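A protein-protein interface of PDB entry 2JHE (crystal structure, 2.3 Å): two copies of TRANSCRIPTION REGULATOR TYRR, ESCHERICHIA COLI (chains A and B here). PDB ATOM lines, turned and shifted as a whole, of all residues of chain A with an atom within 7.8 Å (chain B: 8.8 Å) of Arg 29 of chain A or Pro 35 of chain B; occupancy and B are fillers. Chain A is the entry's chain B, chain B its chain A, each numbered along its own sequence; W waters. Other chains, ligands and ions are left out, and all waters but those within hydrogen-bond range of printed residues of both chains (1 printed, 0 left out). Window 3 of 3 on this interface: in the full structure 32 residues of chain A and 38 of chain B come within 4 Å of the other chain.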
ATOM      1  N   MET A   1     -24.647  31.479  -0.811  1.00  0.00           N
ATOM      2  CA  MET A   1     -24.482  30.884   0.519  1.00  0.00           C
ATOM      3  C   MET A   1     -23.039  30.434   0.600  1.00  0.00           C
ATOM      4  O   MET A   1     -22.509  29.802  -0.309  1.00  0.00           O
ATOM      5  CB  MET A   1     -25.450  29.711   0.690  1.00  0.00           C
ATOM      6  CG  MET A   1     -26.252  29.754   1.970  1.00  0.00           C
ATOM      7  SD  MET A   1     -27.947  29.051   1.897  1.00  0.00           S
ATOM      8  CE  MET A   1     -27.595  27.365   1.659  1.00  0.00           C
ATOM      9  N   LEU A  21     -21.504  17.245   0.438  1.00  0.00           N
ATOM     10  CA  LEU A  21     -22.269  18.167  -0.387  1.00  0.00           C
ATOM     11  C   LEU A  21     -22.752  17.523  -1.682  1.00  0.00           C
ATOM     12  O   LEU A  21     -23.918  17.701  -2.065  1.00  0.00           O
ATOM     13  CB  LEU A  21     -21.482  19.485  -0.621  1.00  0.00           C
ATOM     14  CG  LEU A  21     -21.636  20.517   0.535  1.00  0.00           C
ATOM     15  CD1 LEU A  21     -20.558  20.319   1.565  1.00  0.00           C
ATOM     16  CD2 LEU A  21     -21.496  21.932   0.023  1.00  0.00           C
ATOM     17  N   ILE A  26     -26.092  19.287  -3.002  1.00  0.00           N
ATOM     18  CA  ILE A  26     -25.799  20.732  -2.951  1.00  0.00           C
ATOM     19  C   ILE A  26     -25.058  21.230  -4.200  1.00  0.00           C
ATOM     20  O   ILE A  26     -24.092  20.629  -4.679  1.00  0.00           O
ATOM     21  CB  ILE A  26     -25.075  21.107  -1.662  1.00  0.00           C
ATOM     22  CG1 ILE A  26     -26.006  20.841  -0.487  1.00  0.00           C
ATOM     23  CG2 ILE A  26     -24.589  22.583  -1.669  1.00  0.00           C
ATOM     24  CD1 ILE A  26     -25.330  20.246   0.632  1.00  0.00           C
ATOM     25  N   ASP A  27     -25.554  22.338  -4.731  1.00  0.00           N
ATOM     26  CA  ASP A  27     -25.033  22.906  -5.960  1.00  0.00           C
ATOM     27  C   ASP A  27     -23.800  23.709  -5.570  1.00  0.00           C
ATOM     28  O   ASP A  27     -23.898  24.927  -5.377  1.00  0.00           O
ATOM     29  CB  ASP A  27     -26.137  23.792  -6.563  1.00  0.00           C
ATOM     30  CG  ASP A  27     -25.785  24.360  -7.922  1.00  0.00           C
ATOM     31  OD1 ASP A  27     -24.618  24.231  -8.360  1.00  0.00           O
ATOM     32  OD2 ASP A  27     -26.712  24.952  -8.536  1.00  0.00           O
ATOM     33  N   LEU A  28     -22.661  22.996  -5.424  1.00  0.00           N
ATOM     34  CA  LEU A  28     -21.385  23.594  -5.088  1.00  0.00           C
ATOM     35  C   LEU A  28     -20.722  24.347  -6.259  1.00  0.00           C
ATOM     36  O   LEU A  28     -20.501  23.791  -7.323  1.00  0.00           O
ATOM     37  CB  LEU A  28     -20.415  22.556  -4.534  1.00  0.00           C
ATOM     38  CG  LEU A  28     -19.055  23.051  -4.021  1.00  0.00           C
ATOM     39  CD1 LEU A  28     -19.148  23.982  -2.789  1.00  0.00           C
ATOM     40  CD2 LEU A  28     -18.266  21.799  -3.754  1.00  0.00           C
ATOM     41  N   ARG A  29     -20.418  25.627  -6.036  1.00  0.00           N
ATOM     42  CA  ARG A  29     -19.784  26.454  -7.054  1.00  0.00           C
ATOM     43  C   ARG A  29     -18.308  26.589  -6.727  1.00  0.00           C
ATOM     44  O   ARG A  29     -17.463  26.549  -7.620  1.00  0.00           O
ATOM     45  CB  ARG A  29     -20.458  27.808  -7.169  1.00  0.00           C
ATOM     46  CG  ARG A  29     -21.865  27.771  -7.704  1.00  0.00           C
ATOM     47  CD  ARG A  29     -22.037  26.782  -8.915  1.00  0.00           C
ATOM     48  NE  ARG A  29     -23.483  26.541  -9.112  1.00  0.00           N
ATOM     49  CZ  ARG A  29     -24.292  27.305  -9.851  1.00  0.00           C
ATOM     50  NH1 ARG A  29     -23.821  28.351 -10.551  1.00  0.00           N
ATOM     51  NH2 ARG A  29     -25.574  27.038  -9.886  1.00  0.00           N
ATOM     52  N   GLY A  30     -17.967  26.717  -5.451  1.00  0.00           N
ATOM     53  CA  GLY A  30     -16.557  26.944  -5.129  1.00  0.00           C
ATOM     54  C   GLY A  30     -16.096  26.509  -3.777  1.00  0.00           C
ATOM     55  O   GLY A  30     -16.848  26.530  -2.788  1.00  0.00           O
ATOM     56  N   ILE A  31     -14.850  26.077  -3.757  1.00  0.00           N
ATOM     57  CA  ILE A  31     -14.144  25.809  -2.491  1.00  0.00           C
ATOM     58  C   ILE A  31     -12.836  26.632  -2.513  1.00  0.00           C
ATOM     59  O   ILE A  31     -12.143  26.677  -3.525  1.00  0.00           O
ATOM     60  CB  ILE A  31     -13.800  24.271  -2.314  1.00  0.00           C
ATOM     61  CG1 ILE A  31     -15.091  23.446  -2.259  1.00  0.00           C
ATOM     62  CG2 ILE A  31     -12.993  24.001  -1.048  1.00  0.00           C
ATOM     63  CD1 ILE A  31     -14.871  21.896  -2.029  1.00  0.00           C
ATOM     64  N   LEU A  41     -16.700  27.494   1.455  1.00  0.00           N
ATOM     65  CA  LEU A  41     -17.624  26.830   0.523  1.00  0.00           C
ATOM     66  C   LEU A  41     -18.595  27.851  -0.027  1.00  0.00           C
ATOM     67  O   LEU A  41     -19.168  28.609   0.727  1.00  0.00           O
ATOM     68  CB  LEU A  41     -18.464  25.749   1.255  1.00  0.00           C
ATOM     69  CG  LEU A  41     -17.758  24.627   2.046  1.00  0.00           C
ATOM     70  CD1 LEU A  41     -18.800  23.752   2.805  1.00  0.00           C
ATOM     71  CD2 LEU A  41     -16.808  23.740   1.160  1.00  0.00           C
ATOM     72  N   ASN A  42     -18.786  27.833  -1.334  1.00  0.00           N
ATOM     73  CA  ASN A  42     -19.707  28.718  -1.996  1.00  0.00           C
ATOM     74  C   ASN A  42     -20.687  27.867  -2.797  1.00  0.00           C
ATOM     75  O   ASN A  42     -20.288  27.164  -3.702  1.00  0.00           O
ATOM     76  CB  ASN A  42     -18.959  29.671  -2.964  1.00  0.00           C
ATOM     77  CG  ASN A  42     -19.807  30.889  -3.374  1.00  0.00           C
ATOM     78  OD1 ASN A  42     -20.993  31.019  -3.045  1.00  0.00           O
ATOM     79  ND2 ASN A  42     -19.180  31.800  -4.047  1.00  0.00           N
ATOM     80  N   PHE A  43     -21.966  27.945  -2.468  1.00  0.00           N
ATOM     81  CA  PHE A  43     -22.924  27.101  -3.125  1.00  0.00           C
ATOM     82  C   PHE A  43     -24.231  27.836  -3.334  1.00  0.00           C
ATOM     83  O   PHE A  43     -24.513  28.852  -2.656  1.00  0.00           O
ATOM     84  CB  PHE A  43     -23.127  25.789  -2.312  1.00  0.00           C
ATOM     85  CG  PHE A  43     -23.367  26.003  -0.846  1.00  0.00           C
ATOM     86  CD1 PHE A  43     -24.637  26.220  -0.371  1.00  0.00           C
ATOM     87  CD2 PHE A  43     -22.317  25.972   0.065  1.00  0.00           C
ATOM     88  CE1 PHE A  43     -24.850  26.397   0.977  1.00  0.00           C
ATOM     89  CE2 PHE A  43     -22.529  26.205   1.429  1.00  0.00           C
ATOM     90  CZ  PHE A  43     -23.785  26.377   1.876  1.00  0.00           C
ATOM     91  N   ALA A  44     -25.045  27.308  -4.249  1.00  0.00           N
ATOM     92  CA  ALA A  44     -26.386  27.895  -4.531  1.00  0.00           C
ATOM     93  C   ALA A  44     -27.288  27.900  -3.288  1.00  0.00           C
ATOM     94  O   ALA A  44     -27.024  27.190  -2.305  1.00  0.00           O
ATOM     95  CB  ALA A  44     -27.081  27.174  -5.703  1.00  0.00           C
ATOM     96  N   GLU A  45     -28.319  28.743  -3.325  1.00  0.00           N
ATOM     97  CA  GLU A  45     -29.185  28.981  -2.200  1.00  0.00           C
ATOM     98  C   GLU A  45     -29.876  27.693  -1.751  1.00  0.00           C
ATOM     99  O   GLU A  45     -30.398  26.933  -2.567  1.00  0.00           O
ATOM    100  CB  GLU A  45     -30.218  30.081  -2.504  1.00  0.00           C
ATOM    101  CG  GLU A  45     -29.614  31.496  -2.667  1.00  0.00           C
ATOM    102  CD  GLU A  45     -28.472  31.811  -1.649  1.00  0.00           C
ATOM    103  OE1 GLU A  45     -28.813  32.073  -0.447  1.00  0.00           O
ATOM    104  OE2 GLU A  45     -27.264  31.813  -2.070  1.00  0.00           O
ATOM    105  N   MET A  73     -16.132  35.003   0.349  1.00  0.00           N
ATOM    106  CA  MET A  73     -14.966  34.138   0.156  1.00  0.00           C
ATOM    107  C   MET A  73     -13.680  34.962   0.289  1.00  0.00           C
ATOM    108  O   MET A  73     -13.707  36.184   0.117  1.00  0.00           O
ATOM    109  CB  MET A  73     -15.033  33.418  -1.221  1.00  0.00           C
ATOM    110  CG  MET A  73     -16.279  32.523  -1.493  1.00  0.00           C
ATOM    111  SD  MET A  73     -16.392  31.010  -0.439  1.00  0.00           S
ATOM    112  CE  MET A  73     -15.430  29.943  -1.496  1.00  0.00           C
ATOM    113  N   CYS B   7     -15.873  17.795 -18.630  1.00  0.00           N
ATOM    114  CA  CYS B   7     -16.270  16.489 -18.208  1.00  0.00           C
ATOM    115  C   CYS B   7     -17.734  16.328 -18.460  1.00  0.00           C
ATOM    116  O   CYS B   7     -18.470  17.311 -18.567  1.00  0.00           O
ATOM    117  CB  CYS B   7     -15.940  16.314 -16.715  1.00  0.00           C
ATOM    118  SG  CYS B   7     -16.730  17.629 -15.720  1.00  0.00           S
ATOM    119  N   GLU B   8     -18.169  15.084 -18.575  1.00  0.00           N
ATOM    120  CA  GLU B   8     -19.579  14.894 -18.565  1.00  0.00           C
ATOM    121  C   GLU B   8     -20.092  14.871 -17.136  1.00  0.00           C
ATOM    122  O   GLU B   8     -19.346  14.986 -16.191  1.00  0.00           O
ATOM    123  CB  GLU B   8     -20.017  13.707 -19.424  1.00  0.00           C
ATOM    124  CG  GLU B   8     -19.240  12.437 -19.248  1.00  0.00           C
ATOM    125  CD  GLU B   8     -18.862  11.828 -20.605  1.00  0.00           C
ATOM    126  OE1 GLU B   8     -19.049  12.518 -21.649  1.00  0.00           O
ATOM    127  OE2 GLU B   8     -18.377  10.672 -20.624  1.00  0.00           O
ATOM    128  N   ASP B   9     -21.399  14.752 -17.026  1.00  0.00           N
ATOM    129  CA  ASP B   9     -22.155  14.783 -15.803  1.00  0.00           C
ATOM    130  C   ASP B   9     -22.078  13.440 -15.083  1.00  0.00           C
ATOM    131  O   ASP B   9     -23.026  12.646 -15.148  1.00  0.00           O
ATOM    132  CB  ASP B   9     -23.624  15.137 -16.159  1.00  0.00           C
ATOM    133  CG  ASP B   9     -24.116  14.470 -17.484  1.00  0.00           C
ATOM    134  OD1 ASP B   9     -23.324  14.346 -18.460  1.00  0.00           O
ATOM    135  OD2 ASP B   9     -25.309  14.081 -17.569  1.00  0.00           O
ATOM    136  N   GLY B  30      -7.940  25.521  -4.343  1.00  0.00           N
ATOM    137  CA  GLY B  30      -9.273  25.833  -4.757  1.00  0.00           C
ATOM    138  C   GLY B  30      -9.787  24.909  -5.828  1.00  0.00           C
ATOM    139  O   GLY B  30      -9.045  24.477  -6.731  1.00  0.00           O
ATOM    140  N   ILE B  31     -11.077  24.627  -5.759  1.00  0.00           N
ATOM    141  CA  ILE B  31     -11.754  23.932  -6.836  1.00  0.00           C
ATOM    142  C   ILE B  31     -13.054  24.673  -7.051  1.00  0.00           C
ATOM    143  O   ILE B  31     -13.732  25.004  -6.099  1.00  0.00           O
ATOM    144  CB  ILE B  31     -11.935  22.387  -6.565  1.00  0.00           C
ATOM    145  CG1 ILE B  31     -12.980  21.804  -7.483  1.00  0.00           C
ATOM    146  CG2 ILE B  31     -12.366  22.112  -5.155  1.00  0.00           C
ATOM    147  CD1 ILE B  31     -12.930  20.279  -7.631  1.00  0.00           C
ATOM    148  N   GLU B  32     -13.339  25.006  -8.306  1.00  0.00           N
ATOM    149  CA  GLU B  32     -14.625  25.627  -8.712  1.00  0.00           C
ATOM    150  C   GLU B  32     -15.298  24.796  -9.789  1.00  0.00           C
ATOM    151  O   GLU B  32     -14.645  24.109 -10.557  1.00  0.00           O
ATOM    152  CB  GLU B  32     -14.414  27.086  -9.172  1.00  0.00           C
ATOM    153  CG  GLU B  32     -13.842  27.825  -7.960  1.00  0.00           C
ATOM    154  CD  GLU B  32     -13.394  29.258  -8.175  1.00  0.00           C
ATOM    155  OE1 GLU B  32     -13.714  29.895  -9.207  1.00  0.00           O
ATOM    156  OE2 GLU B  32     -12.730  29.740  -7.234  1.00  0.00           O
ATOM    157  N   ILE B  33     -16.606  24.871  -9.824  1.00  0.00           N
ATOM    158  CA  ILE B  33     -17.441  24.038 -10.683  1.00  0.00           C
ATOM    159  C   ILE B  33     -18.454  24.899 -11.425  1.00  0.00           C
ATOM    160  O   ILE B  33     -19.144  25.736 -10.838  1.00  0.00           O
ATOM    161  CB  ILE B  33     -18.217  22.992  -9.849  1.00  0.00           C
ATOM    162  CG1 ILE B  33     -17.247  22.004  -9.202  1.00  0.00           C
ATOM    163  CG2 ILE B  33     -19.358  22.298 -10.685  1.00  0.00           C
ATOM    164  CD1 ILE B  33     -17.885  21.315  -8.016  1.00  0.00           C
ATOM    165  N   ASP B  34     -18.501  24.659 -12.730  1.00  0.00           N
ATOM    166  CA  ASP B  34     -19.514  25.151 -13.634  1.00  0.00           C
ATOM    167  C   ASP B  34     -20.453  23.951 -13.964  1.00  0.00           C
ATOM    168  O   ASP B  34     -20.038  22.978 -14.662  1.00  0.00           O
ATOM    169  CB  ASP B  34     -18.799  25.613 -14.913  1.00  0.00           C
ATOM    170  CG  ASP B  34     -19.495  26.716 -15.604  1.00  0.00           C
ATOM    171  OD1 ASP B  34     -20.714  26.912 -15.369  1.00  0.00           O
ATOM    172  OD2 ASP B  34     -18.805  27.394 -16.417  1.00  0.00           O
ATOM    173  N   PRO B  35     -21.710  24.014 -13.488  1.00  0.00           N
ATOM    174  CA  PRO B  35     -22.818  23.093 -13.814  1.00  0.00           C
ATOM    175  C   PRO B  35     -22.910  22.659 -15.298  1.00  0.00           C
ATOM    176  O   PRO B  35     -23.485  21.595 -15.586  1.00  0.00           O
ATOM    177  CB  PRO B  35     -24.080  23.940 -13.501  1.00  0.00           C
ATOM    178  CG  PRO B  35     -23.533  25.368 -13.191  1.00  0.00           C
ATOM    179  CD  PRO B  35     -22.184  25.095 -12.614  1.00  0.00           C
ATOM    180  N   ILE B  36     -22.394  23.486 -16.214  1.00  0.00           N
ATOM    181  CA  ILE B  36     -22.375  23.178 -17.649  1.00  0.00           C
ATOM    182  C   ILE B  36     -21.472  21.982 -17.948  1.00  0.00           C
ATOM    183  O   ILE B  36     -21.741  21.200 -18.859  1.00  0.00           O
ATOM    184  CB  ILE B  36     -21.945  24.417 -18.479  1.00  0.00           C
ATOM    185  N   GLY B  37     -20.418  21.806 -17.168  1.00  0.00           N
ATOM    186  CA  GLY B  37     -19.531  20.669 -17.378  1.00  0.00           C
ATOM    187  C   GLY B  37     -18.065  21.061 -17.254  1.00  0.00           C
ATOM    188  O   GLY B  37     -17.238  20.560 -18.019  1.00  0.00           O
ATOM    189  N   ARG B  38     -17.734  21.946 -16.300  1.00  0.00           N
ATOM    190  CA  ARG B  38     -16.328  22.376 -16.159  1.00  0.00           C
ATOM    191  C   ARG B  38     -15.899  22.506 -14.725  1.00  0.00           C
ATOM    192  O   ARG B  38     -16.604  23.106 -13.870  1.00  0.00           O
ATOM    193  CB  ARG B  38     -16.062  23.728 -16.874  1.00  0.00           C
ATOM    194  CG  ARG B  38     -16.341  23.799 -18.367  1.00  0.00           C
ATOM    195  CD  ARG B  38     -16.635  25.238 -18.739  1.00  0.00           C
ATOM    196  NE  ARG B  38     -17.010  25.426 -20.146  1.00  0.00           N
ATOM    197  CZ  ARG B  38     -16.865  26.571 -20.815  1.00  0.00           C
ATOM    198  NH1 ARG B  38     -16.323  27.628 -20.236  1.00  0.00           N
ATOM    199  NH2 ARG B  38     -17.223  26.662 -22.080  1.00  0.00           N
ATOM    200  N   ILE B  39     -14.716  21.975 -14.465  1.00  0.00           N
ATOM    201  CA  ILE B  39     -14.136  21.984 -13.140  1.00  0.00           C
ATOM    202  C   ILE B  39     -12.765  22.756 -13.220  1.00  0.00           C
ATOM    203  O   ILE B  39     -11.885  22.392 -14.022  1.00  0.00           O
ATOM    204  CB  ILE B  39     -13.932  20.507 -12.623  1.00  0.00           C
ATOM    205  CG1 ILE B  39     -15.263  19.783 -12.517  1.00  0.00           C
ATOM    206  CG2 ILE B  39     -13.231  20.478 -11.270  1.00  0.00           C
ATOM    207  CD1 ILE B  39     -15.166  18.360 -11.893  1.00  0.00           C
ATOM    208  N   TYR B  40     -12.599  23.795 -12.399  1.00  0.00           N
ATOM    209  CA  TYR B  40     -11.318  24.524 -12.323  1.00  0.00           C
ATOM    210  C   TYR B  40     -10.575  24.135 -11.079  1.00  0.00           C
ATOM    211  O   TYR B  40     -11.173  23.948 -10.036  1.00  0.00           O
ATOM    212  CB  TYR B  40     -11.538  26.047 -12.378  1.00  0.00           C
ATOM    213  CG  TYR B  40     -12.310  26.518 -13.589  1.00  0.00           C
ATOM    214  CD1 TYR B  40     -13.719  26.500 -13.614  1.00  0.00           C
ATOM    215  CD2 TYR B  40     -11.637  26.982 -14.710  1.00  0.00           C
ATOM    216  CE1 TYR B  40     -14.436  26.944 -14.754  1.00  0.00           C
ATOM    217  CE2 TYR B  40     -12.331  27.459 -15.846  1.00  0.00           C
ATOM    218  CZ  TYR B  40     -13.721  27.439 -15.858  1.00  0.00           C
ATOM    219  OH  TYR B  40     -14.383  27.933 -17.002  1.00  0.00           O
ATOM    220  N   MET B  73      -8.857  31.118 -12.068  1.00  0.00           N
ATOM    221  CA  MET B  73     -10.157  30.617 -11.633  1.00  0.00           C
ATOM    222  C   MET B  73     -11.282  31.636 -11.902  1.00  0.00           C
ATOM    223  O   MET B  73     -11.064  32.845 -11.829  1.00  0.00           O
ATOM    224  CB  MET B  73     -10.144  30.344 -10.103  1.00  0.00           C
ATOM    225  CG  MET B  73      -8.970  29.525  -9.632  1.00  0.00           C
ATOM    226  SD  MET B  73      -9.111  27.844 -10.251  1.00  0.00           S
ATOM    227  CE  MET B  73     -10.286  27.267  -9.016  1.00  0.00           C
ATOM    228  N   PRO B  74     -12.525  31.145 -12.145  1.00  0.00           N
ATOM    229  CA  PRO B  74     -13.620  32.138 -12.187  1.00  0.00           C
ATOM    230  C   PRO B  74     -13.547  33.146 -11.037  1.00  0.00           C
ATOM    231  O   PRO B  74     -13.790  34.321 -11.274  1.00  0.00           O
ATOM    232  CB  PRO B  74     -14.902  31.272 -12.075  1.00  0.00           C
ATOM    233  CG  PRO B  74     -14.496  29.961 -12.718  1.00  0.00           C
ATOM    234  CD  PRO B  74     -13.007  29.761 -12.367  1.00  0.00           C
ATOM    235  N   SER B  75     -13.251  32.686  -9.804  1.00  0.00           N
ATOM    236  CA  SER B  75     -13.150  33.591  -8.619  1.00  0.00           C
ATOM    237  C   SER B  75     -12.036  34.674  -8.673  1.00  0.00           C
ATOM    238  O   SER B  75     -12.160  35.702  -8.022  1.00  0.00           O
ATOM    239  CB  SER B  75     -12.968  32.778  -7.347  1.00  0.00           C
ATOM    240  OG  SER B  75     -11.813  31.947  -7.444  1.00  0.00           O
HETATM  241  O   HOH W   1     -11.093  28.248  -5.890  1.00  0.00           O
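The backbone carbonyl oxygen (O) of Arg 29 of chain A is in hydrogen-bond range of the backbone NH (N) of Ile 33 of chain B (2.9 Å). The backbone carbonyl oxygen (O) of Ile 31 of chain B sits at hydrogen-bond distance from the backbone NH (N) of Ile 31 of chain A, 2.8 Å away.
OD1 of Asp 27 of chain A is in salt-bridge range of NE of Arg 29 of chain A, 2.7 Å away. The backbone carbonyl oxygen (O) of Gly 30 of chain A lies within hydrogen-bond range of the backbone NH (N) of Asn 42 of chain A, at 2.8 Å. O of Glu 32 of chain B lies within hydrogen-bond range of N of Tyr 40 of chain B (2.8 Å). The side-chain carboxylate (OE1) of Glu 32 of chain B is in hydrogen-bond range of the backbone NH (N) of Ser 75 of chain B (2.9 Å). N of Arg 29 of chain A is in hydrogen-bond range of O of Asn 42 of chain A, 2.8 Å away.
Among the printed residues, merely in contact across the chains: Arg 29 of chain A with Glu 32 of chain B, Ile 31 of chain A with Gly 30 of chain B, Leu 28 of chain A with Ile 33 of chain B, Gly 30 of chain A with Ile 31 of chain B and Arg 29 of chain A with Pro 35 of chain B.
Arg 29 of chain A touches three residues of chain B. Pro 35 of chain B touches just one residue of chain A: Arg 29 (3.9 Å). Gly 30 of chain A touches just one residue of chain B: Ile 31 (3.6 Å). Printed residues of chain A within 4 Å of Ile 33 of chain B: Leu 28 (3.5 Å) and Arg 29 (2.9 Å). Of the printed residues of chain B, Ile 31 of chain A touches Gly 30 (3.2 Å) and Ile 31 (2.8 Å). Leu 21 of chain A touches none of the printed residues of chain B. Asn 42 of chain A touches none of the printed residues of chain B. The nearest residue of chain B that does not touch Arg 29 of chain A is Ile 31 of chain B (4.3 Å). The nearest residue of chain A that does not touch Pro 35 of chain B is Asp 27 of chain A (5.0 Å).
Of the 14 printed residues of chain A, 4 touch a printed residue of chain B. Hydrophobic or aromatic side chains of chain A that line the printed part of chain B: Ile 31. Of the 17 printed residues of chain B, 5 touch a printed residue of chain A. Hydrophobic or aromatic side chains of chain B that line the printed part of chain A: Ile 31, Ile 33 and Pro 35. Among the printed residues, no Asp or Glu carboxylate lies within 4 Å of a Lys or Arg side-chain nitrogen of the other chain.
Gly 30 of chain A touches Ile 31 of chain B, and with the chains exchanged Ile 31 of chain A touches Gly 30 of chain B. Ile 31 of chain B touches its own counterpart, Ile 31 of chain A. Positions printed for both chains: 30, 31 and 73. Of the 7 pairs that touch across the chains among the printed residues, 3 have their exchanged pair printed and touching as well.
Water W1 lies within hydrogen-bond range of the side-chain carboxylate of Glu 32 of chain B and the backbone carbonyl oxygen of Ile 31 of chain A.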
